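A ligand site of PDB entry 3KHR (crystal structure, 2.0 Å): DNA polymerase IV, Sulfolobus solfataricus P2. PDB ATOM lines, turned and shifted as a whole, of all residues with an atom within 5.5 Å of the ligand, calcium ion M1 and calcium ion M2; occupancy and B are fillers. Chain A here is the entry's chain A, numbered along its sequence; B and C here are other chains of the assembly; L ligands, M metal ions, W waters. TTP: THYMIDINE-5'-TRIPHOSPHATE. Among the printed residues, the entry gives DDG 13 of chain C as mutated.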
ATOM      1  N   ASP A   7      11.941 -13.502  31.190  1.00  0.00           N
ATOM      2  CA  ASP A   7      11.158 -13.706  29.976  1.00  0.00           C
ATOM      3  C   ASP A   7      10.383 -15.040  30.209  1.00  0.00           C
ATOM      4  O   ASP A   7      11.001 -16.117  30.392  1.00  0.00           O
ATOM      5  CB  ASP A   7      12.136 -13.753  28.788  1.00  0.00           C
ATOM      6  CG  ASP A   7      11.458 -13.978  27.435  1.00  0.00           C
ATOM      7  OD1 ASP A   7      10.441 -14.674  27.413  1.00  0.00           O
ATOM      8  OD2 ASP A   7      11.986 -13.509  26.376  1.00  0.00           O
ATOM      9  N   PHE A   8       9.043 -14.974  30.233  1.00  0.00           N
ATOM     10  CA  PHE A   8       8.224 -16.125  30.651  1.00  0.00           C
ATOM     11  C   PHE A   8       8.173 -17.133  29.513  1.00  0.00           C
ATOM     12  O   PHE A   8       8.068 -16.720  28.368  1.00  0.00           O
ATOM     13  CB  PHE A   8       6.772 -15.741  31.046  1.00  0.00           C
ATOM     14  CG  PHE A   8       6.665 -14.558  31.987  1.00  0.00           C
ATOM     15  CD1 PHE A   8       7.730 -14.138  32.768  1.00  0.00           C
ATOM     16  CD2 PHE A   8       5.451 -13.890  32.110  1.00  0.00           C
ATOM     17  CE1 PHE A   8       7.619 -13.021  33.630  1.00  0.00           C
ATOM     18  CE2 PHE A   8       5.321 -12.773  32.956  1.00  0.00           C
ATOM     19  CZ  PHE A   8       6.412 -12.351  33.717  1.00  0.00           C
ATOM     20  N   ASP A   9       8.257 -18.438  29.816  1.00  0.00           N
ATOM     21  CA  ASP A   9       8.397 -19.461  28.757  1.00  0.00           C
ATOM     22  C   ASP A   9       7.059 -19.751  28.057  1.00  0.00           C
ATOM     23  O   ASP A   9       6.034 -19.960  28.708  1.00  0.00           O
ATOM     24  CB  ASP A   9       8.982 -20.795  29.289  1.00  0.00           C
ATOM     25  CG  ASP A   9      10.370 -20.653  29.933  1.00  0.00           C
ATOM     26  OD1 ASP A   9      11.234 -19.880  29.455  1.00  0.00           O
ATOM     27  OD2 ASP A   9      10.606 -21.333  30.960  1.00  0.00           O
ATOM     28  N   TYR A  10       7.079 -19.797  26.726  1.00  0.00           N
ATOM     29  CA  TYR A  10       5.906 -20.030  25.869  1.00  0.00           C
ATOM     30  C   TYR A  10       4.609 -19.521  26.495  1.00  0.00           C
ATOM     31  O   TYR A  10       3.629 -20.264  26.657  1.00  0.00           O
ATOM     32  CB  TYR A  10       5.815 -21.505  25.405  1.00  0.00           C
ATOM     33  CG  TYR A  10       5.718 -22.567  26.523  1.00  0.00           C
ATOM     34  CD1 TYR A  10       4.513 -23.270  26.741  1.00  0.00           C
ATOM     35  CD2 TYR A  10       6.820 -22.881  27.304  1.00  0.00           C
ATOM     36  CE1 TYR A  10       4.431 -24.241  27.732  1.00  0.00           C
ATOM     37  CE2 TYR A  10       6.745 -23.837  28.300  1.00  0.00           C
ATOM     38  CZ  TYR A  10       5.555 -24.509  28.505  1.00  0.00           C
ATOM     39  OH  TYR A  10       5.514 -25.435  29.503  1.00  0.00           O
ATOM     40  N   PHE A  11       4.612 -18.227  26.860  1.00  0.00           N
ATOM     41  CA  PHE A  11       3.715 -17.744  27.921  1.00  0.00           C
ATOM     42  C   PHE A  11       2.236 -18.139  27.817  1.00  0.00           C
ATOM     43  O   PHE A  11       1.740 -18.770  28.742  1.00  0.00           O
ATOM     44  CB  PHE A  11       3.909 -16.225  28.186  1.00  0.00           C
ATOM     45  CG  PHE A  11       3.139 -15.710  29.370  1.00  0.00           C
ATOM     46  CD1 PHE A  11       3.130 -16.409  30.582  1.00  0.00           C
ATOM     47  CD2 PHE A  11       2.427 -14.520  29.266  1.00  0.00           C
ATOM     48  CE1 PHE A  11       2.408 -15.931  31.672  1.00  0.00           C
ATOM     49  CE2 PHE A  11       1.679 -14.022  30.348  1.00  0.00           C
ATOM     50  CZ  PHE A  11       1.678 -14.717  31.557  1.00  0.00           C
ATOM     51  N   TYR A  12       1.528 -17.766  26.746  1.00  0.00           N
ATOM     52  CA  TYR A  12       0.075 -18.019  26.672  1.00  0.00           C
ATOM     53  C   TYR A  12      -0.258 -19.511  26.740  1.00  0.00           C
ATOM     54  O   TYR A  12      -1.178 -19.920  27.471  1.00  0.00           O
ATOM     55  CB  TYR A  12      -0.539 -17.426  25.394  1.00  0.00           C
ATOM     56  CG  TYR A  12      -0.560 -15.913  25.299  1.00  0.00           C
ATOM     57  CD1 TYR A  12       0.034 -15.122  26.265  1.00  0.00           C
ATOM     58  CD2 TYR A  12      -1.167 -15.293  24.196  1.00  0.00           C
ATOM     59  CE1 TYR A  12       0.021 -13.720  26.142  1.00  0.00           C
ATOM     60  CE2 TYR A  12      -1.163 -13.918  24.053  1.00  0.00           C
ATOM     61  CZ  TYR A  12      -0.591 -13.137  25.039  1.00  0.00           C
ATOM     62  OH  TYR A  12      -0.620 -11.769  24.897  1.00  0.00           O
ATOM     63  N   ALA A  13       0.469 -20.318  25.972  1.00  0.00           N
ATOM     64  CA  ALA A  13       0.282 -21.768  25.980  1.00  0.00           C
ATOM     65  C   ALA A  13       0.577 -22.381  27.360  1.00  0.00           C
ATOM     66  O   ALA A  13      -0.172 -23.262  27.838  1.00  0.00           O
ATOM     67  CB  ALA A  13       1.180 -22.425  24.886  1.00  0.00           C
ATOM     68  N   VAL A  43      -1.722 -17.576  14.593  1.00  0.00           N
ATOM     69  CA  VAL A  43      -1.251 -18.147  15.849  1.00  0.00           C
ATOM     70  C   VAL A  43      -0.597 -17.079  16.703  1.00  0.00           C
ATOM     71  O   VAL A  43       0.255 -16.337  16.215  1.00  0.00           O
ATOM     72  CB  VAL A  43      -0.213 -19.288  15.559  1.00  0.00           C
ATOM     73  CG1 VAL A  43       0.491 -19.729  16.833  1.00  0.00           C
ATOM     74  CG2 VAL A  43      -0.887 -20.482  14.864  1.00  0.00           C
ATOM     75  N   ALA A  44      -0.943 -17.010  17.986  1.00  0.00           N
ATOM     76  CA  ALA A  44      -0.275 -16.089  18.916  1.00  0.00           C
ATOM     77  C   ALA A  44       1.014 -16.705  19.450  1.00  0.00           C
ATOM     78  O   ALA A  44       2.038 -15.998  19.575  1.00  0.00           O
ATOM     79  CB  ALA A  44      -1.216 -15.679  20.087  1.00  0.00           C
ATOM     80  N   THR A  45       0.950 -17.983  19.829  1.00  0.00           N
ATOM     81  CA  THR A  45       2.139 -18.743  20.227  1.00  0.00           C
ATOM     82  C   THR A  45       1.828 -20.235  20.288  1.00  0.00           C
ATOM     83  O   THR A  45       0.681 -20.626  20.092  1.00  0.00           O
ATOM     84  CB  THR A  45       2.736 -18.310  21.609  1.00  0.00           C
ATOM     85  OG1 THR A  45       4.016 -18.923  21.765  1.00  0.00           O
ATOM     86  CG2 THR A  45       1.857 -18.771  22.762  1.00  0.00           C
ATOM     87  N   ALA A  46       2.852 -21.049  20.560  1.00  0.00           N
ATOM     88  CA  ALA A  46       2.607 -22.473  20.733  1.00  0.00           C
ATOM     89  C   ALA A  46       3.662 -23.009  21.663  1.00  0.00           C
ATOM     90  O   ALA A  46       4.751 -22.427  21.765  1.00  0.00           O
ATOM     91  CB  ALA A  46       2.661 -23.209  19.392  1.00  0.00           C
ATOM     92  N   TYR A  48       6.524 -25.776  23.079  1.00  0.00           N
ATOM     93  CA  TYR A  48       7.691 -26.269  22.374  1.00  0.00           C
ATOM     94  C   TYR A  48       7.422 -27.555  21.608  1.00  0.00           C
ATOM     95  O   TYR A  48       8.030 -27.795  20.562  1.00  0.00           O
ATOM     96  CB  TYR A  48       8.896 -26.366  23.326  1.00  0.00           C
ATOM     97  CG  TYR A  48       9.539 -25.007  23.512  1.00  0.00           C
ATOM     98  CD1 TYR A  48       8.966 -24.053  24.355  1.00  0.00           C
ATOM     99  CD2 TYR A  48      10.705 -24.667  22.813  1.00  0.00           C
ATOM    100  CE1 TYR A  48       9.535 -22.781  24.523  1.00  0.00           C
ATOM    101  CE2 TYR A  48      11.294 -23.384  22.983  1.00  0.00           C
ATOM    102  CZ  TYR A  48      10.702 -22.451  23.838  1.00  0.00           C
ATOM    103  OH  TYR A  48      11.267 -21.193  24.010  1.00  0.00           O
ATOM    104  N   ARG A  51       6.160 -26.483  18.310  1.00  0.00           N
ATOM    105  CA  ARG A  51       7.176 -25.774  17.514  1.00  0.00           C
ATOM    106  C   ARG A  51       8.093 -26.716  16.769  1.00  0.00           C
ATOM    107  O   ARG A  51       8.655 -26.330  15.742  1.00  0.00           O
ATOM    108  CB  ARG A  51       8.013 -24.823  18.368  1.00  0.00           C
ATOM    109  CG  ARG A  51       7.203 -23.662  18.956  1.00  0.00           C
ATOM    110  CD  ARG A  51       8.099 -22.749  19.789  1.00  0.00           C
ATOM    111  NE  ARG A  51       7.282 -21.968  20.725  1.00  0.00           N
ATOM    112  CZ  ARG A  51       7.730 -20.974  21.472  1.00  0.00           C
ATOM    113  NH1 ARG A  51       9.008 -20.577  21.384  1.00  0.00           N
ATOM    114  NH2 ARG A  51       6.883 -20.344  22.284  1.00  0.00           N
ATOM    115  N   ALA A  57       4.420 -18.339  16.365  1.00  0.00           N
ATOM    116  CA  ALA A  57       3.688 -17.083  16.370  1.00  0.00           C
ATOM    117  C   ALA A  57       3.550 -16.489  14.963  1.00  0.00           C
ATOM    118  O   ALA A  57       4.511 -16.471  14.198  1.00  0.00           O
ATOM    119  CB  ALA A  57       4.372 -16.082  17.339  1.00  0.00           C
ATOM    120  N   GLY A  58       2.351 -16.075  14.580  1.00  0.00           N
ATOM    121  CA  GLY A  58       2.147 -15.347  13.335  1.00  0.00           C
ATOM    122  C   GLY A  58       1.735 -16.126  12.097  1.00  0.00           C
ATOM    123  O   GLY A  58       1.216 -15.538  11.147  1.00  0.00           O
ATOM    124  N   MET A  76      -7.184 -17.543  21.975  1.00  0.00           N
ATOM    125  CA  MET A  76      -6.387 -16.691  22.868  1.00  0.00           C
ATOM    126  C   MET A  76      -7.310 -15.965  23.854  1.00  0.00           C
ATOM    127  O   MET A  76      -8.237 -15.268  23.427  1.00  0.00           O
ATOM    128  CB  MET A  76      -5.558 -15.687  22.049  1.00  0.00           C
ATOM    129  CG  MET A  76      -4.701 -14.760  22.892  1.00  0.00           C
ATOM    130  SD  MET A  76      -4.133 -13.297  22.024  1.00  0.00           S
ATOM    131  CE  MET A  76      -5.652 -12.445  21.595  1.00  0.00           C
ATOM    132  N   SER A 103       6.900  -5.834  28.367  1.00  0.00           N
ATOM    133  CA  SER A 103       5.742  -6.392  27.652  1.00  0.00           C
ATOM    134  C   SER A 103       4.944  -7.267  28.601  1.00  0.00           C
ATOM    135  O   SER A 103       5.276  -7.347  29.790  1.00  0.00           O
ATOM    136  CB  SER A 103       6.187  -7.256  26.483  1.00  0.00           C
ATOM    137  OG  SER A 103       6.867  -8.390  26.996  1.00  0.00           O
ATOM    138  N   ILE A 104       3.938  -7.979  28.091  1.00  0.00           N
ATOM    139  CA  ILE A 104       3.145  -8.883  28.915  1.00  0.00           C
ATOM    140  C   ILE A 104       4.010  -9.960  29.623  1.00  0.00           C
ATOM    141  O   ILE A 104       3.614 -10.472  30.659  1.00  0.00           O
ATOM    142  CB  ILE A 104       1.962  -9.551  28.129  1.00  0.00           C
ATOM    143  CG1 ILE A 104       0.889 -10.062  29.100  1.00  0.00           C
ATOM    144  CG2 ILE A 104       2.478 -10.668  27.195  1.00  0.00           C
ATOM    145  CD1 ILE A 104      -0.503 -10.178  28.526  1.00  0.00           C
ATOM    146  N   ASP A 105       5.176 -10.271  29.090  1.00  0.00           N
ATOM    147  CA  ASP A 105       5.969 -11.372  29.698  1.00  0.00           C
ATOM    148  C   ASP A 105       7.487 -11.146  29.854  1.00  0.00           C
ATOM    149  O   ASP A 105       8.252 -12.111  29.981  1.00  0.00           O
ATOM    150  CB  ASP A 105       5.659 -12.711  28.970  1.00  0.00           C
ATOM    151  CG  ASP A 105       6.565 -12.958  27.770  1.00  0.00           C
ATOM    152  OD1 ASP A 105       6.977 -11.976  27.132  1.00  0.00           O
ATOM    153  OD2 ASP A 105       6.894 -14.134  27.491  1.00  0.00           O
ATOM    154  N   GLU A 106       7.891  -9.871  29.882  1.00  0.00           N
ATOM    155  CA  GLU A 106       9.297  -9.458  30.006  1.00  0.00           C
ATOM    156  C   GLU A 106       9.441  -8.350  31.012  1.00  0.00           C
ATOM    157  O   GLU A 106       8.682  -7.377  30.957  1.00  0.00           O
ATOM    158  CB  GLU A 106       9.806  -8.845  28.701  1.00  0.00           C
ATOM    159  CG  GLU A 106       9.821  -9.706  27.502  1.00  0.00           C
ATOM    160  CD  GLU A 106      10.302  -8.954  26.290  1.00  0.00           C
ATOM    161  OE1 GLU A 106       9.837  -7.810  26.038  1.00  0.00           O
ATOM    162  OE2 GLU A 106      11.148  -9.511  25.558  1.00  0.00           O
ATOM    163  N   LYS A 152      19.024  -9.608  27.496  1.00  0.00           N
ATOM    164  CA  LYS A 152      17.977 -10.193  26.675  1.00  0.00           C
ATOM    165  C   LYS A 152      18.561 -11.314  25.806  1.00  0.00           C
ATOM    166  O   LYS A 152      17.961 -12.395  25.676  1.00  0.00           O
ATOM    167  CB  LYS A 152      17.305  -9.125  25.795  1.00  0.00           C
ATOM    168  CG  LYS A 152      16.106  -9.653  25.000  1.00  0.00           C
ATOM    169  CD  LYS A 152      15.487  -8.541  24.178  1.00  0.00           C
ATOM    170  CE  LYS A 152      13.995  -8.454  24.369  1.00  0.00           C
ATOM    171  NZ  LYS A 152      13.280  -9.574  23.744  1.00  0.00           N
ATOM    172  N   LYS A 159      16.742 -20.167  26.716  1.00  0.00           N
ATOM    173  CA  LYS A 159      15.314 -20.526  26.553  1.00  0.00           C
ATOM    174  C   LYS A 159      15.151 -22.002  26.168  1.00  0.00           C
ATOM    175  O   LYS A 159      15.962 -22.489  25.387  1.00  0.00           O
ATOM    176  CB  LYS A 159      14.666 -19.666  25.446  1.00  0.00           C
ATOM    177  CG  LYS A 159      14.070 -18.363  25.893  1.00  0.00           C
ATOM    178  CD  LYS A 159      13.199 -17.728  24.789  1.00  0.00           C
ATOM    179  CE  LYS A 159      12.961 -16.227  25.075  1.00  0.00           C
ATOM    180  NZ  LYS A 159      11.857 -15.574  24.273  1.00  0.00           N
ATOM    181  N   PRO A 160      14.141 -22.724  26.705  1.00  0.00           N
ATOM    182  CA  PRO A 160      13.188 -22.373  27.786  1.00  0.00           C
ATOM    183  C   PRO A 160      13.691 -22.826  29.164  1.00  0.00           C
ATOM    184  O   PRO A 160      14.627 -23.621  29.244  1.00  0.00           O
ATOM    185  CB  PRO A 160      11.936 -23.177  27.405  1.00  0.00           C
ATOM    186  CG  PRO A 160      12.493 -24.446  26.756  1.00  0.00           C
ATOM    187  CD  PRO A 160      13.819 -24.038  26.105  1.00  0.00           C
ATOM    188  P    DA B   4      -4.166 -11.236   9.609  1.00  0.00           P
ATOM    189  OP1  DA B   4      -5.481 -11.181   8.922  1.00  0.00           O
ATOM    190  OP2  DA B   4      -3.198 -10.129   9.510  1.00  0.00           O
ATOM    191  O5'  DA B   4      -4.395 -11.565  11.149  1.00  0.00           O
ATOM    192  C5'  DA B   4      -5.348 -12.552  11.538  1.00  0.00           C
ATOM    193  C4'  DA B   4      -5.791 -12.253  12.948  1.00  0.00           C
ATOM    194  O4'  DA B   4      -4.756 -12.580  13.908  1.00  0.00           O
ATOM    195  C3'  DA B   4      -6.085 -10.786  13.208  1.00  0.00           C
ATOM    196  O3'  DA B   4      -7.161 -10.744  14.105  1.00  0.00           O
ATOM    197  C2'  DA B   4      -4.800 -10.201  13.807  1.00  0.00           C
ATOM    198  C1'  DA B   4      -4.185 -11.427  14.497  1.00  0.00           C
ATOM    199  N9   DA B   4      -2.740 -11.593  14.353  1.00  0.00           N
ATOM    200  C8   DA B   4      -1.999 -11.607  13.215  1.00  0.00           C
ATOM    201  N7   DA B   4      -0.714 -11.802  13.426  1.00  0.00           N
ATOM    202  C5   DA B   4      -0.612 -11.927  14.802  1.00  0.00           C
ATOM    203  C6   DA B   4       0.487 -12.167  15.685  1.00  0.00           C
ATOM    204  N6   DA B   4       1.763 -12.295  15.274  1.00  0.00           N
ATOM    205  N1   DA B   4       0.240 -12.246  17.017  1.00  0.00           N
ATOM    206  C2   DA B   4      -1.018 -12.096  17.437  1.00  0.00           C
ATOM    207  N3   DA B   4      -2.114 -11.902  16.695  1.00  0.00           N
ATOM    208  C4   DA B   4      -1.848 -11.811  15.387  1.00  0.00           C
ATOM    209  P    DC B   5      -7.972  -9.370  14.302  1.00  0.00           P
ATOM    210  OP1  DC B   5      -9.272  -9.733  14.900  1.00  0.00           O
ATOM    211  OP2  DC B   5      -7.929  -8.633  13.025  1.00  0.00           O
ATOM    212  O5'  DC B   5      -7.068  -8.586  15.349  1.00  0.00           O
ATOM    213  C5'  DC B   5      -6.892  -9.107  16.682  1.00  0.00           C
ATOM    214  C4'  DC B   5      -5.761  -8.381  17.396  1.00  0.00           C
ATOM    215  O4'  DC B   5      -4.470  -8.945  17.004  1.00  0.00           O
ATOM    216  C3'  DC B   5      -5.675  -6.868  17.112  1.00  0.00           C
ATOM    217  O3'  DC B   5      -5.312  -6.110  18.274  1.00  0.00           O
ATOM    218  C2'  DC B   5      -4.466  -6.783  16.171  1.00  0.00           C
ATOM    219  C1'  DC B   5      -3.603  -7.839  16.874  1.00  0.00           C
ATOM    220  N1   DC B   5      -2.321  -8.118  16.206  1.00  0.00           N
ATOM    221  C2   DC B   5      -1.226  -8.479  17.024  1.00  0.00           C
ATOM    222  O2   DC B   5      -1.371  -8.544  18.251  1.00  0.00           O
ATOM    223  N3   DC B   5      -0.021  -8.704  16.434  1.00  0.00           N
ATOM    224  C4   DC B   5       0.102  -8.613  15.109  1.00  0.00           C
ATOM    225  N4   DC B   5       1.310  -8.854  14.587  1.00  0.00           N
ATOM    226  C5   DC B   5      -1.006  -8.261  14.255  1.00  0.00           C
ATOM    227  C6   DC B   5      -2.178  -7.995  14.856  1.00  0.00           C
ATOM    228  P   DDG C  13      10.580  -9.110  21.599  1.00  0.00           P
ATOM    229  OP1 DDG C  13      11.253  -7.874  22.078  1.00  0.00           O
ATOM    230  OP2 DDG C  13      11.321 -10.353  21.370  1.00  0.00           O
ATOM    231  O5' DDG C  13       9.373  -9.535  22.561  1.00  0.00           O
ATOM    232  C5' DDG C  13       8.656  -8.609  23.296  1.00  0.00           C
ATOM    233  C4' DDG C  13       7.192  -8.984  23.377  1.00  0.00           C
ATOM    234  O4' DDG C  13       6.529  -8.396  22.248  1.00  0.00           O
ATOM    235  C3' DDG C  13       6.834 -10.460  23.200  1.00  0.00           C
ATOM    236  C2' DDG C  13       5.347 -10.370  22.910  1.00  0.00           C
ATOM    237  C1' DDG C  13       5.320  -9.118  22.048  1.00  0.00           C
ATOM    238  N9  DDG C  13       5.232  -9.287  20.611  1.00  0.00           N
ATOM    239  C8  DDG C  13       6.216  -9.474  19.673  1.00  0.00           C
ATOM    240  N7  DDG C  13       5.748  -9.540  18.448  1.00  0.00           N
ATOM    241  C5  DDG C  13       4.377  -9.390  18.603  1.00  0.00           C
ATOM    242  C6  DDG C  13       3.342  -9.359  17.654  1.00  0.00           C
ATOM    243  O6  DDG C  13       3.438  -9.482  16.425  1.00  0.00           O
ATOM    244  N1  DDG C  13       2.096  -9.191  18.250  1.00  0.00           N
ATOM    245  C2  DDG C  13       1.880  -9.045  19.611  1.00  0.00           C
ATOM    246  N2  DDG C  13       0.629  -8.890  20.051  1.00  0.00           N
ATOM    247  N3  DDG C  13       2.845  -9.061  20.505  1.00  0.00           N
ATOM    248  C4  DDG C  13       4.053  -9.238  19.923  1.00  0.00           C
HETATM  249  PA  TTP L   1       7.357 -14.354  23.382  1.00  0.00           P
HETATM  250  O1A TTP L   1       8.170 -14.109  24.630  1.00  0.00           O
HETATM  251  O2A TTP L   1       7.968 -13.901  22.093  1.00  0.00           O
HETATM  252  O3A TTP L   1       6.986 -15.892  23.084  1.00  0.00           O
HETATM  253  PB  TTP L   1       6.627 -17.032  24.157  1.00  0.00           P
HETATM  254  O1B TTP L   1       6.694 -16.622  25.605  1.00  0.00           O
HETATM  255  O2B TTP L   1       5.326 -17.670  23.750  1.00  0.00           O
HETATM  256  O3B TTP L   1       7.744 -18.125  23.774  1.00  0.00           O
HETATM  257  PG  TTP L   1       9.267 -18.170  24.268  1.00  0.00           P
HETATM  258  O1G TTP L   1       9.499 -19.353  25.174  1.00  0.00           O
HETATM  259  O2G TTP L   1      10.077 -18.483  23.052  1.00  0.00           O
HETATM  260  O3G TTP L   1       9.705 -16.911  24.973  1.00  0.00           O
HETATM  261  O5' TTP L   1       5.908 -13.681  23.452  1.00  0.00           O
HETATM  262  C5' TTP L   1       5.182 -13.652  24.690  1.00  0.00           C
HETATM  263  C4' TTP L   1       3.711 -13.794  24.389  1.00  0.00           C
HETATM  264  O4' TTP L   1       3.246 -12.735  23.550  1.00  0.00           O
HETATM  265  C3' TTP L   1       3.398 -15.100  23.664  1.00  0.00           C
HETATM  266  O3' TTP L   1       3.249 -16.205  24.571  1.00  0.00           O
HETATM  267  C2' TTP L   1       2.104 -14.751  22.928  1.00  0.00           C
HETATM  268  C1' TTP L   1       2.247 -13.240  22.659  1.00  0.00           C
HETATM  269  N1  TTP L   1       2.678 -13.065  21.252  1.00  0.00           N
HETATM  270  C2  TTP L   1       1.705 -12.763  20.267  1.00  0.00           C
HETATM  271  O2  TTP L   1       0.497 -12.661  20.586  1.00  0.00           O
HETATM  272  N3  TTP L   1       2.075 -12.614  18.986  1.00  0.00           N
HETATM  273  C4  TTP L   1       3.350 -12.753  18.589  1.00  0.00           C
HETATM  274  O4  TTP L   1       3.668 -12.615  17.392  1.00  0.00           O
HETATM  275  C5  TTP L   1       4.399 -13.057  19.603  1.00  0.00           C
HETATM  276  C5M TTP L   1       5.848 -13.212  19.248  1.00  0.00           C
HETATM  277  C6  TTP L   1       3.972 -13.201  20.924  1.00  0.00           C
HETATM  278 CA    CA M   1       8.902 -12.039  25.474  1.00  0.00          CA
HETATM  279 CA    CA M   2       8.504 -15.479  26.482  1.00  0.00          CA
HETATM  280  O   HOH W   1      11.057 -11.700  24.853  1.00  0.00           O
HETATM  281  O   HOH W   2       5.597 -12.876  15.632  1.00  0.00           O
HETATM  282  O   HOH W   3      10.522 -17.117  21.089  1.00  0.00           O
HETATM  283  O   HOH W   4       6.439 -16.808  20.396  1.00  0.00           O
HETATM  284  O   HOH W   5      11.211 -17.586  27.436  1.00  0.00           O
HETATM  285  O   HOH W   6      -1.011 -11.069  22.213  1.00  0.00           O
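O6 of DDG 13 of chain C sits close to an oxygen (O4) of the ligand, 3.3 Å away.
Merely in contact with the ligand: Ala 57 and Asp 9.
Hydrophobic or aromatic side chains within 4 Å of the ligand: Phe 11, Tyr 12, Ala 44, Tyr 48 and Ala 57.
The nearest printed residue that does not touch the ligand is Ile 104 (4.3 Å).
Calcium ion M2 is bound by the side-chain carboxylate (OD1) of Asp 7 (2.3 Å), the backbone carbonyl oxygen (O) of Phe 8 (2.3 Å), an oxygen (O1B) of the ligand (2.3 Å), the side-chain carboxylate (OD2) of Asp 105 (2.3 Å), an oxygen (O1A) of the ligand (2.3 Å) and an oxygen (O3G) of the ligand (2.4 Å).
The side-chain carboxylate (OD2) of Asp 7 lies within salt-bridge range of the side-chain amino group (NZ) of Lys 159, at 3.0 Å.
The side-chain hydroxyl of Ser 103 lies close to the backbone NH of Asp 105, at 3.3 Å.
The side-chain hydroxyl (OG1) of Thr 45 is in hydrogen-bond range of the guanidinium group (NH2) of Arg 51 (3.2 Å).
The backbone carbonyl oxygen (O) of Ala 46 is in hydrogen-bond range of the guanidinium group (NE) of Arg 51.
OE1 of Glu 106 is in hydrogen-bond range of OG of Ser 103.
The side-chain amino group of Lys 152 lies within salt-bridge range of the side-chain carboxylate of Glu 106 (2.8 Å).
N2 of DDG 13 of chain C lies close to O2 of DC 5 of chain B (2.7 Å).
OP1 of DDG 13 of chain C is in salt-bridge range of NZ of Lys 152, at 3.1 Å.
Water W1 bridges the side-chain carboxylate (OD2) of Asp 7 (2.5 Å) and the side-chain amino group (NZ) of Lys 152 (3.3 Å).
Water W6 lies within hydrogen-bond range of an oxygen (O2) of the ligand (2.7 Å), the side-chain hydroxyl of Tyr 12 (2.8 Å) and N2 of DDG 13 of chain C (3.5 Å).
Water W4 bridges O3A of the ligand (2.9 Å) and OG1 of Thr 45 (3.5 Å).
Water W5 lies within hydrogen-bond range of the side-chain carboxylate (OD1) of Asp 9, the backbone carbonyl oxygen (O) of Asp 7 and an oxygen (O1G) of the ligand.
The side-chain amino group of Lys 159 is in salt-bridge range of an oxygen (O2G) of the ligand (3.6 Å).
OG1 of Thr 45 is in hydrogen-bond range of O2B of the ligand, 2.7 Å away.
N1 of DA 4 of chain B sits at hydrogen-bond distance from a nitrogen (N3) of the ligand.
An oxygen (O1G) of the ligand sits at hydrogen-bond distance from the side-chain hydroxyl (OH) of Tyr 48 (2.8 Å).
The guanidinium group (NH1) of Arg 51 lies within salt-bridge range of an oxygen (O2G) of the ligand (2.9 Å).
The backbone NH (N) of Tyr 10 is in hydrogen-bond range of an oxygen (O1G) of the ligand (2.9 Å).
An oxygen (O2B) of the ligand lies within hydrogen-bond range of the backbone NH (N) of Phe 11 (3.2 Å).
The backbone NH of Tyr 12 sits at hydrogen-bond distance from an oxygen (O3') of the ligand (3.2 Å).
The backbone carbonyl oxygen (O) of Ala 44 sits close to a nitrogen (N3) of the ligand (3.4 Å).
Merely in contact with calcium ion M1: Glu 106 and DDG 13 of chain C.
Four residues have an atom within 4 Å of calcium ion M1: Asp 7, Asp 105, Glu 106 and DDG 13 of chain C.
The nearest printed residue that does not touch calcium ion M1 is Ser 103 (4.4 Å).
Within 4 Å of calcium ion M2: Asp 7, Phe 8 and Asp 105.
Along chain A the residues within 4 Å of calcium ion M2 span positions 7 to 105.
The nearest printed residue that does not touch calcium ion M2 is Lys 159 (4.02 Å).
Calcium ion M1 is bound by water W1 (2.3 Å).
Calcium ion M1 is bound by an oxygen (O1A) of the ligand (2.4 Å).
OD1 of Asp 105 is bound to calcium ion M1 (2.5 Å).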
